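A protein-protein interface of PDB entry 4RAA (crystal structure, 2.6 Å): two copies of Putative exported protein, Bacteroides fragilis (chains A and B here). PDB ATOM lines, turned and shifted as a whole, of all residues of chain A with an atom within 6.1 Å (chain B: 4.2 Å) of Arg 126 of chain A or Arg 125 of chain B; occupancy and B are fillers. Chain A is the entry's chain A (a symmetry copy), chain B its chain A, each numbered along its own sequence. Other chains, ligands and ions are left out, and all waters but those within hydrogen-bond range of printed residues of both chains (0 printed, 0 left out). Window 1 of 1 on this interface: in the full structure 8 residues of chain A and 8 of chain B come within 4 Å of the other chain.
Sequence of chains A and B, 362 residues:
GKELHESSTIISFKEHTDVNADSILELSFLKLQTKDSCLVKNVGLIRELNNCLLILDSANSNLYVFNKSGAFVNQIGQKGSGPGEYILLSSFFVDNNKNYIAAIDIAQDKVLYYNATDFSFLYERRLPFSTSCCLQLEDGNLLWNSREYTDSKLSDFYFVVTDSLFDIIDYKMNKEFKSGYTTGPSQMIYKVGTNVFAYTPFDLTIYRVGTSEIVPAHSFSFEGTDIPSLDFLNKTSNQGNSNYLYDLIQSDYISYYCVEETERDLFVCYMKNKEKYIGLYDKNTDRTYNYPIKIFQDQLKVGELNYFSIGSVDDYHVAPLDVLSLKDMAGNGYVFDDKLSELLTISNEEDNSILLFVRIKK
The guanidinium group (NE) of Arg 126 of chain B sits close to the backbone carbonyl oxygen (O) of Leu 165 of chain A, at 3.4 Å.
The backbone carbonyl oxygen (O) of Leu 165 of chain B lies close to the guanidinium group (NE) of Arg 126 of chain A (3.4 Å).
The side-chain carboxylate of Asp 167 of chain B is in salt-bridge range of the guanidinium group of Arg 126 of chain A, 3.1 Å away.
Printed residues of chain B that touch a printed residue of chain A: Tyr 123, Glu 124, Arg 125, Arg 126, Pro 128, Leu 165, Phe 166 and Asp 167.
Hydrophobic or aromatic side chains of chain B within 4 Å of the printed part of chain A: Tyr 123, Pro 128, Leu 165 and Phe 166.
Of the 12 printed residues of chain A, 7 touch a printed residue of chain B.
Printed residues of chain A that touch a printed residue of chain B: Tyr 123, Glu 124, Arg 125, Arg 126, Pro 128, Leu 165 and Phe 166.
Of chain B, only Arg 125 (3.9 Å), Pro 128 (3.6 Å), Leu 165 (3.4 Å), Phe 166 (3.5 Å) and Asp 167 (3.1 Å) come within 4 Å of Arg 126 of chain A.
Of chain A, only Glu 124 (3.97 Å), Arg 125 (3.7 Å) and Arg 126 (3.9 Å) come within 4 Å of Arg 125 of chain B.
Printed residues of chain B within 4 Å of Leu 165 of chain A: Glu 124 and Arg 126.
Of the printed residues of chain A, Arg 126 of chain B touches Arg 125 (3.9 Å), Pro 128 (3.6 Å), Leu 165 (3.4 Å) and Phe 166 (3.5 Å).
Printed residues of chain A within 4 Å of Leu 165 of chain B: Glu 124 (3.8 Å) and Arg 126 (3.4 Å).
Printed residues of chain B within 4 Å of Phe 166 of chain A: Arg 126 (3.5 Å).
The nearest printed residue of chain B that does not touch Arg 126 of chain A is Arg 126 of chain B (5.3 Å).
The nearest printed residue of chain B that does not touch Phe 166 of chain A is Glu 124 of chain B (7.3 Å).
The side-chain amino group (NZ) of Lys 110 of chain B is in salt-bridge range of the side-chain carboxylate (OE1) of Glu 124 of chain B, at 2.8 Å.
O of Arg 125 of chain B is in hydrogen-bond range of N of Val 111 of chain B (2.7 Å).
O of Leu 165 of chain B sits at hydrogen-bond distance from NH2 of Arg 125 of chain B (2.8 Å).
NZ of Lys 110 of chain A is in salt-bridge range of OE1 of Glu 124 of chain A (2.8 Å).
N of Val 111 of chain A is in hydrogen-bond range of O of Arg 125 of chain A, at 2.7 Å.
O of Leu 165 of chain A is in hydrogen-bond range of NH2 of Arg 125 of chain A (2.8 Å).
Among the printed residues, pairs that only touch across the chains: Tyr 123 of chain A with Tyr 123 of chain B, Phe 166 of chain A with Arg 126 of chain B, Arg 126 of chain A with Phe 166 of chain B, Arg 126 of chain A with Pro 128 of chain B, Pro 128 of chain A with Arg 126 of chain B, Arg 125 of chain A with Arg 125 of chain B, Glu 124 of chain A with Leu 165 of chain B, Leu 165 of chain A with Glu 124 of chain B, Arg 126 of chain A with Arg 125 of chain B, Arg 125 of chain A with Arg 126 of chain B, Arg 125 of chain A with Glu 124 of chain B and Glu 124 of chain A with Arg 125 of chain B.
Glu 124 of chain A touches Arg 125 of chain B, and with the chains exchanged Arg 125 of chain A touches Glu 124 of chain B.
Arg 126 of chain A touches Pro 128 of chain B, and with the chains exchanged Pro 128 of chain A touches Arg 126 of chain B.
Arg 126 of chain A touches Leu 165 of chain B, and with the chains exchanged Leu 165 of chain A touches Arg 126 of chain B.
Arg 126 of chain A touches Phe 166 of chain B, and with the chains exchanged Phe 166 of chain A touches Arg 126 of chain B.
Positions printed for both chains: 110, 111, 123, 124, 125, 126, 127, 128, 165 and 166.
Of the 15 pairs that touch across the chains among the printed residues, 14 have their exchanged pair printed and touching as well.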
ATOM      1  N   ASP A 109      11.882  25.187 -13.403  1.00  0.00           N
ATOM      2  CA  ASP A 109      12.521  26.360 -14.040  1.00  0.00           C
ATOM      3  C   ASP A 109      12.571  26.275 -15.559  1.00  0.00           C
ATOM      4  O   ASP A 109      13.631  26.436 -16.175  1.00  0.00           O
ATOM      5  CB  ASP A 109      13.914  26.615 -13.434  1.00  0.00           C
ATOM      6  CG  ASP A 109      13.837  27.116 -12.010  1.00  0.00           C
ATOM      7  OD1 ASP A 109      13.396  28.280 -11.833  1.00  0.00           O
ATOM      8  OD2 ASP A 109      14.234  26.366 -11.086  1.00  0.00           O
ATOM      9  N   LYS A 110      11.404  25.992 -16.141  1.00  0.00           N
ATOM     10  CA  LYS A 110      11.252  25.894 -17.594  1.00  0.00           C
ATOM     11  C   LYS A 110       9.902  26.394 -18.117  1.00  0.00           C
ATOM     12  O   LYS A 110       8.942  26.541 -17.367  1.00  0.00           O
ATOM     13  CB  LYS A 110      11.521  24.463 -18.068  1.00  0.00           C
ATOM     14  CG  LYS A 110      10.689  23.385 -17.388  1.00  0.00           C
ATOM     15  CD  LYS A 110      10.812  22.066 -18.146  1.00  0.00           C
ATOM     16  CE  LYS A 110      10.011  20.956 -17.478  1.00  0.00           C
ATOM     17  NZ  LYS A 110       9.947  19.691 -18.268  1.00  0.00           N
ATOM     18  N   VAL A 111       9.886  26.663 -19.417  1.00  0.00           N
ATOM     19  CA  VAL A 111       8.728  27.121 -20.176  1.00  0.00           C
ATOM     20  C   VAL A 111       8.444  25.999 -21.161  1.00  0.00           C
ATOM     21  O   VAL A 111       9.361  25.580 -21.868  1.00  0.00           O
ATOM     22  CB  VAL A 111       9.062  28.389 -21.009  1.00  0.00           C
ATOM     23  CG1 VAL A 111       7.820  28.925 -21.709  1.00  0.00           C
ATOM     24  CG2 VAL A 111       9.657  29.472 -20.126  1.00  0.00           C
ATOM     25  N   TYR A 123       8.213  22.238 -27.968  1.00  0.00           N
ATOM     26  CA  TYR A 123       9.568  22.344 -27.386  1.00  0.00           C
ATOM     27  C   TYR A 123       9.557  22.995 -26.016  1.00  0.00           C
ATOM     28  O   TYR A 123       8.555  23.597 -25.638  1.00  0.00           O
ATOM     29  CB  TYR A 123      10.499  23.159 -28.292  1.00  0.00           C
ATOM     30  CG  TYR A 123      10.142  24.629 -28.451  1.00  0.00           C
ATOM     31  CD1 TYR A 123       9.131  25.038 -29.327  1.00  0.00           C
ATOM     32  CD2 TYR A 123      10.841  25.619 -27.741  1.00  0.00           C
ATOM     33  CE1 TYR A 123       8.816  26.386 -29.485  1.00  0.00           C
ATOM     34  CE2 TYR A 123      10.538  26.967 -27.888  1.00  0.00           C
ATOM     35  CZ  TYR A 123       9.532  27.352 -28.759  1.00  0.00           C
ATOM     36  OH  TYR A 123       9.250  28.697 -28.890  1.00  0.00           O
ATOM     37  N   GLU A 124      10.668  22.876 -25.283  1.00  0.00           N
ATOM     38  CA  GLU A 124      10.800  23.492 -23.948  1.00  0.00           C
ATOM     39  C   GLU A 124      12.120  24.229 -23.808  1.00  0.00           C
ATOM     40  O   GLU A 124      13.144  23.779 -24.323  1.00  0.00           O
ATOM     41  CB  GLU A 124      10.644  22.464 -22.806  1.00  0.00           C
ATOM     42  CG  GLU A 124      11.733  21.386 -22.711  1.00  0.00           C
ATOM     43  CD  GLU A 124      11.520  20.372 -21.590  1.00  0.00           C
ATOM     44  OE1 GLU A 124      10.501  20.423 -20.870  1.00  0.00           O
ATOM     45  OE2 GLU A 124      12.392  19.492 -21.435  1.00  0.00           O
ATOM     46  N   ARG A 125      12.075  25.348 -23.088  1.00  0.00           N
ATOM     47  CA  ARG A 125      13.243  26.186 -22.801  1.00  0.00           C
ATOM     48  C   ARG A 125      13.303  26.473 -21.315  1.00  0.00           C
ATOM     49  O   ARG A 125      12.302  26.321 -20.622  1.00  0.00           O
ATOM     50  CB  ARG A 125      13.119  27.521 -23.514  1.00  0.00           C
ATOM     51  CG  ARG A 125      13.034  27.429 -25.013  1.00  0.00           C
ATOM     52  CD  ARG A 125      12.963  28.828 -25.606  1.00  0.00           C
ATOM     53  NE  ARG A 125      14.146  29.627 -25.287  1.00  0.00           N
ATOM     54  CZ  ARG A 125      14.248  30.945 -25.410  1.00  0.00           C
ATOM     55  NH1 ARG A 125      13.228  31.689 -25.843  1.00  0.00           N
ATOM     56  NH2 ARG A 125      15.387  31.543 -25.066  1.00  0.00           N
ATOM     57  N   ARG A 126      14.459  26.927 -20.838  1.00  0.00           N
ATOM     58  CA  ARG A 126      14.608  27.295 -19.429  1.00  0.00           C
ATOM     59  C   ARG A 126      14.125  28.715 -19.224  1.00  0.00           C
ATOM     60  O   ARG A 126      14.254  29.557 -20.123  1.00  0.00           O
ATOM     61  CB  ARG A 126      16.054  27.209 -18.967  1.00  0.00           C
ATOM     62  CG  ARG A 126      16.595  25.806 -18.998  1.00  0.00           C
ATOM     63  CD  ARG A 126      18.059  25.774 -18.632  1.00  0.00           C
ATOM     64  NE  ARG A 126      18.898  26.524 -19.566  1.00  0.00           N
ATOM     65  CZ  ARG A 126      20.223  26.643 -19.468  1.00  0.00           C
ATOM     66  NH1 ARG A 126      20.899  26.051 -18.477  1.00  0.00           N
ATOM     67  NH2 ARG A 126      20.886  27.358 -20.384  1.00  0.00           N
ATOM     68  N   LEU A 127      13.575  28.970 -18.034  1.00  0.00           N
ATOM     69  CA  LEU A 127      13.162  30.303 -17.652  1.00  0.00           C
ATOM     70  C   LEU A 127      14.424  31.131 -17.605  1.00  0.00           C
ATOM     71  O   LEU A 127      15.437  30.654 -17.102  1.00  0.00           O
ATOM     72  CB  LEU A 127      12.540  30.352 -16.257  1.00  0.00           C
ATOM     73  CG  LEU A 127      11.205  29.683 -15.941  1.00  0.00           C
ATOM     74  CD1 LEU A 127      10.939  29.852 -14.454  1.00  0.00           C
ATOM     75  CD2 LEU A 127      10.050  30.252 -16.761  1.00  0.00           C
ATOM     76  N   PRO A 128      14.374  32.360 -18.139  1.00  0.00           N
ATOM     77  CA  PRO A 128      15.563  33.212 -18.128  1.00  0.00           C
ATOM     78  C   PRO A 128      15.991  33.733 -16.734  1.00  0.00           C
ATOM     79  O   PRO A 128      17.156  34.116 -16.550  1.00  0.00           O
ATOM     80  CB  PRO A 128      15.150  34.370 -19.039  1.00  0.00           C
ATOM     81  CG  PRO A 128      13.665  34.450 -18.886  1.00  0.00           C
ATOM     82  CD  PRO A 128      13.196  33.055 -18.699  1.00  0.00           C
ATOM     83  N   PHE A 129      15.052  33.742 -15.785  1.00  0.00           N
ATOM     84  CA  PHE A 129      15.256  34.255 -14.422  1.00  0.00           C
ATOM     85  C   PHE A 129      14.084  33.823 -13.528  1.00  0.00           C
ATOM     86  O   PHE A 129      13.164  33.163 -14.013  1.00  0.00           O
ATOM     87  CB  PHE A 129      15.395  35.797 -14.467  1.00  0.00           C
ATOM     88  CG  PHE A 129      14.470  36.473 -15.456  1.00  0.00           C
ATOM     89  CD1 PHE A 129      13.096  36.567 -15.212  1.00  0.00           C
ATOM     90  CD2 PHE A 129      14.977  37.030 -16.635  1.00  0.00           C
ATOM     91  CE1 PHE A 129      12.243  37.182 -16.123  1.00  0.00           C
ATOM     92  CE2 PHE A 129      14.129  37.663 -17.551  1.00  0.00           C
ATOM     93  CZ  PHE A 129      12.754  37.726 -17.294  1.00  0.00           C
ATOM     94  N   LEU A 165      13.575  35.866 -27.804  1.00  0.00           N
ATOM     95  CA  LEU A 165      14.645  34.976 -27.336  1.00  0.00           C
ATOM     96  C   LEU A 165      14.954  35.047 -25.818  1.00  0.00           C
ATOM     97  O   LEU A 165      15.769  34.257 -25.337  1.00  0.00           O
ATOM     98  CB  LEU A 165      15.901  35.293 -28.205  1.00  0.00           C
ATOM     99  CG  LEU A 165      17.086  34.359 -28.428  1.00  0.00           C
ATOM    100  CD1 LEU A 165      16.642  33.019 -28.983  1.00  0.00           C
ATOM    101  CD2 LEU A 165      18.070  35.001 -29.399  1.00  0.00           C
ATOM    102  N   PHE A 166      14.288  35.951 -25.086  1.00  0.00           N
ATOM    103  CA  PHE A 166      14.426  36.190 -23.612  1.00  0.00           C
ATOM    104  C   PHE A 166      15.547  37.175 -23.174  1.00  0.00           C
ATOM    105  O   PHE A 166      15.784  37.336 -21.964  1.00  0.00           O
ATOM    106  CB  PHE A 166      14.521  34.921 -22.714  1.00  0.00           C
ATOM    107  CG  PHE A 166      13.459  33.862 -22.933  1.00  0.00           C
ATOM    108  CD1 PHE A 166      12.201  34.127 -23.514  1.00  0.00           C
ATOM    109  CD2 PHE A 166      13.683  32.576 -22.394  1.00  0.00           C
ATOM    110  CE1 PHE A 166      11.256  33.103 -23.644  1.00  0.00           C
ATOM    111  CE2 PHE A 166      12.727  31.567 -22.500  1.00  0.00           C
ATOM    112  CZ  PHE A 166      11.516  31.829 -23.125  1.00  0.00           C
ATOM    113  N   LYS B 110      22.886  31.701 -30.271  1.00  0.00           N
ATOM    114  CA  LYS B 110      21.684  30.867 -30.295  1.00  0.00           C
ATOM    115  C   LYS B 110      21.850  29.552 -31.063  1.00  0.00           C
ATOM    116  O   LYS B 110      22.780  29.384 -31.847  1.00  0.00           O
ATOM    117  CB  LYS B 110      20.489  31.660 -30.832  1.00  0.00           C
ATOM    118  CG  LYS B 110      20.695  32.308 -32.193  1.00  0.00           C
ATOM    119  CD  LYS B 110      19.362  32.793 -32.756  1.00  0.00           C
ATOM    120  CE  LYS B 110      19.535  33.471 -34.109  1.00  0.00           C
ATOM    121  NZ  LYS B 110      18.250  33.807 -34.790  1.00  0.00           N
ATOM    122  N   VAL B 111      20.929  28.637 -30.786  1.00  0.00           N
ATOM    123  CA  VAL B 111      20.832  27.316 -31.395  1.00  0.00           C
ATOM    124  C   VAL B 111      19.516  27.336 -32.156  1.00  0.00           C
ATOM    125  O   VAL B 111      18.493  27.681 -31.566  1.00  0.00           O
ATOM    126  CB  VAL B 111      20.722  26.202 -30.318  1.00  0.00           C
ATOM    127  CG1 VAL B 111      20.736  24.820 -30.958  1.00  0.00           C
ATOM    128  CG2 VAL B 111      21.857  26.310 -29.314  1.00  0.00           C
ATOM    129  N   TYR B 123      12.055  25.801 -33.739  1.00  0.00           N
ATOM    130  CA  TYR B 123      12.249  26.761 -32.632  1.00  0.00           C
ATOM    131  C   TYR B 123      13.711  27.108 -32.420  1.00  0.00           C
ATOM    132  O   TYR B 123      14.581  26.415 -32.941  1.00  0.00           O
ATOM    133  CB  TYR B 123      11.696  26.206 -31.313  1.00  0.00           C
ATOM    134  CG  TYR B 123      12.415  24.986 -30.760  1.00  0.00           C
ATOM    135  CD1 TYR B 123      12.161  23.706 -31.263  1.00  0.00           C
ATOM    136  CD2 TYR B 123      13.334  25.109 -29.705  1.00  0.00           C
ATOM    137  CE1 TYR B 123      12.807  22.585 -30.744  1.00  0.00           C
ATOM    138  CE2 TYR B 123      13.986  24.002 -29.177  1.00  0.00           C
ATOM    139  CZ  TYR B 123      13.723  22.742 -29.691  1.00  0.00           C
ATOM    140  OH  TYR B 123      14.381  21.657 -29.150  1.00  0.00           O
ATOM    141  N   GLU B 124      13.973  28.172 -31.656  1.00  0.00           N
ATOM    142  CA  GLU B 124      15.351  28.597 -31.342  1.00  0.00           C
ATOM    143  C   GLU B 124      15.517  28.883 -29.860  1.00  0.00           C
ATOM    144  O   GLU B 124      14.608  29.412 -29.221  1.00  0.00           O
ATOM    145  CB  GLU B 124      15.794  29.823 -32.171  1.00  0.00           C
ATOM    146  CG  GLU B 124      15.043  31.134 -31.898  1.00  0.00           C
ATOM    147  CD  GLU B 124      15.490  32.309 -32.763  1.00  0.00           C
ATOM    148  OE1 GLU B 124      16.360  32.155 -33.646  1.00  0.00           O
ATOM    149  OE2 GLU B 124      14.944  33.413 -32.562  1.00  0.00           O
ATOM    150  N   ARG B 125      16.697  28.546 -29.343  1.00  0.00           N
ATOM    151  CA  ARG B 125      17.074  28.771 -27.944  1.00  0.00           C
ATOM    152  C   ARG B 125      18.425  29.455 -27.892  1.00  0.00           C
ATOM    153  O   ARG B 125      19.163  29.427 -28.873  1.00  0.00           O
ATOM    154  CB  ARG B 125      17.211  27.446 -27.217  1.00  0.00           C
ATOM    155  CG  ARG B 125      15.957  26.616 -27.180  1.00  0.00           C
ATOM    156  CD  ARG B 125      16.212  25.343 -26.385  1.00  0.00           C
ATOM    157  NE  ARG B 125      16.592  25.621 -25.000  1.00  0.00           N
ATOM    158  CZ  ARG B 125      17.147  24.755 -24.160  1.00  0.00           C
ATOM    159  NH1 ARG B 125      17.431  23.504 -24.529  1.00  0.00           N
ATOM    160  NH2 ARG B 125      17.454  25.153 -22.926  1.00  0.00           N
ATOM    161  N   ARG B 126      18.761  30.030 -26.741  1.00  0.00           N
ATOM    162  CA  ARG B 126      20.068  30.664 -26.562  1.00  0.00           C
ATOM    163  C   ARG B 126      21.090  29.615 -26.178  1.00  0.00           C
ATOM    164  O   ARG B 126      20.758  28.633 -25.502  1.00  0.00           O
ATOM    165  CB  ARG B 126      20.042  31.728 -25.475  1.00  0.00           C
ATOM    166  CG  ARG B 126      19.157  32.894 -25.820  1.00  0.00           C
ATOM    167  CD  ARG B 126      19.075  33.877 -24.678  1.00  0.00           C
ATOM    168  NE  ARG B 126      18.488  33.302 -23.468  1.00  0.00           N
ATOM    169  CZ  ARG B 126      18.300  33.965 -22.327  1.00  0.00           C
ATOM    170  NH1 ARG B 126      18.636  35.254 -22.212  1.00  0.00           N
ATOM    171  NH2 ARG B 126      17.754  33.330 -21.283  1.00  0.00           N
ATOM    172  N   LEU B 127      22.335  29.838 -26.611  1.00  0.00           N
ATOM    173  CA  LEU B 127      23.439  28.981 -26.239  1.00  0.00           C
ATOM    174  C   LEU B 127      23.591  29.127 -24.743  1.00  0.00           C
ATOM    175  O   LEU B 127      23.504  30.242 -24.237  1.00  0.00           O
ATOM    176  CB  LEU B 127      24.762  29.416 -26.870  1.00  0.00           C
ATOM    177  CG  LEU B 127      25.007  29.334 -28.374  1.00  0.00           C
ATOM    178  CD1 LEU B 127      26.379  29.926 -28.655  1.00  0.00           C
ATOM    179  CD2 LEU B 127      24.918  27.908 -28.912  1.00  0.00           C
ATOM    180  N   PRO B 128      23.802  28.008 -24.035  1.00  0.00           N
ATOM    181  CA  PRO B 128      23.954  28.081 -22.582  1.00  0.00           C
ATOM    182  C   PRO B 128      25.259  28.753 -22.086  1.00  0.00           C
ATOM    183  O   PRO B 128      25.317  29.212 -20.936  1.00  0.00           O
ATOM    184  CB  PRO B 128      23.910  26.608 -22.170  1.00  0.00           C
ATOM    185  CG  PRO B 128      24.447  25.875 -23.357  1.00  0.00           C
ATOM    186  CD  PRO B 128      23.995  26.636 -24.548  1.00  0.00           C
ATOM    187  N   SER B 164      19.242  17.367 -21.967  1.00  0.00           N
ATOM    188  CA  SER B 164      18.327  17.897 -22.999  1.00  0.00           C
ATOM    189  C   SER B 164      18.139  19.432 -22.905  1.00  0.00           C
ATOM    190  O   SER B 164      18.282  20.162 -23.873  1.00  0.00           O
ATOM    191  CB  SER B 164      16.968  17.177 -22.798  1.00  0.00           C
ATOM    192  OG  SER B 164      15.893  17.706 -23.543  1.00  0.00           O
ATOM    193  N   LEU B 165      17.898  19.887 -21.681  1.00  0.00           N
ATOM    194  CA  LEU B 165      17.554  21.278 -21.356  1.00  0.00           C
ATOM    195  C   LEU B 165      18.757  22.248 -21.225  1.00  0.00           C
ATOM    196  O   LEU B 165      18.540  23.449 -21.055  1.00  0.00           O
ATOM    197  CB  LEU B 165      16.693  21.233 -20.057  1.00  0.00           C
ATOM    198  CG  LEU B 165      15.733  22.321 -19.589  1.00  0.00           C
ATOM    199  CD1 LEU B 165      14.696  22.641 -20.649  1.00  0.00           C
ATOM    200  CD2 LEU B 165      15.024  21.869 -18.318  1.00  0.00           C
ATOM    201  N   PHE B 166      19.990  21.733 -21.339  1.00  0.00           N
ATOM    202  CA  PHE B 166      21.286  22.482 -21.248  1.00  0.00           C
ATOM    203  C   PHE B 166      21.875  22.674 -19.821  1.00  0.00           C
ATOM    204  O   PHE B 166      22.890  23.376 -19.666  1.00  0.00           O
ATOM    205  CB  PHE B 166      21.342  23.855 -21.982  1.00  0.00           C
ATOM    206  CG  PHE B 166      20.880  23.865 -23.426  1.00  0.00           C
ATOM    207  CD1 PHE B 166      20.855  22.716 -24.244  1.00  0.00           C
ATOM    208  CD2 PHE B 166      20.600  25.113 -24.025  1.00  0.00           C
ATOM    209  CE1 PHE B 166      20.454  22.814 -25.582  1.00  0.00           C
ATOM    210  CE2 PHE B 166      20.231  25.209 -25.365  1.00  0.00           C
ATOM    211  CZ  PHE B 166      20.157  24.062 -26.142  1.00  0.00           C
ATOM    212  N   ASP B 167      21.267  22.078 -18.795  1.00  0.00           N
ATOM    213  CA  ASP B 167      21.839  22.117 -17.436  1.00  0.00           C
ATOM    214  C   ASP B 167      23.069  21.195 -17.445  1.00  0.00           C
ATOM    215  O   ASP B 167      23.007  20.089 -17.985  1.00  0.00           O
ATOM    216  CB  ASP B 167      20.823  21.671 -16.377  1.00  0.00           C
ATOM    217  CG  ASP B 167      19.632  22.621 -16.254  1.00  0.00           C
ATOM    218  OD1 ASP B 167      19.754  23.826 -16.581  1.00  0.00           O
ATOM    219  OD2 ASP B 167      18.563  22.154 -15.807  1.00  0.00           O
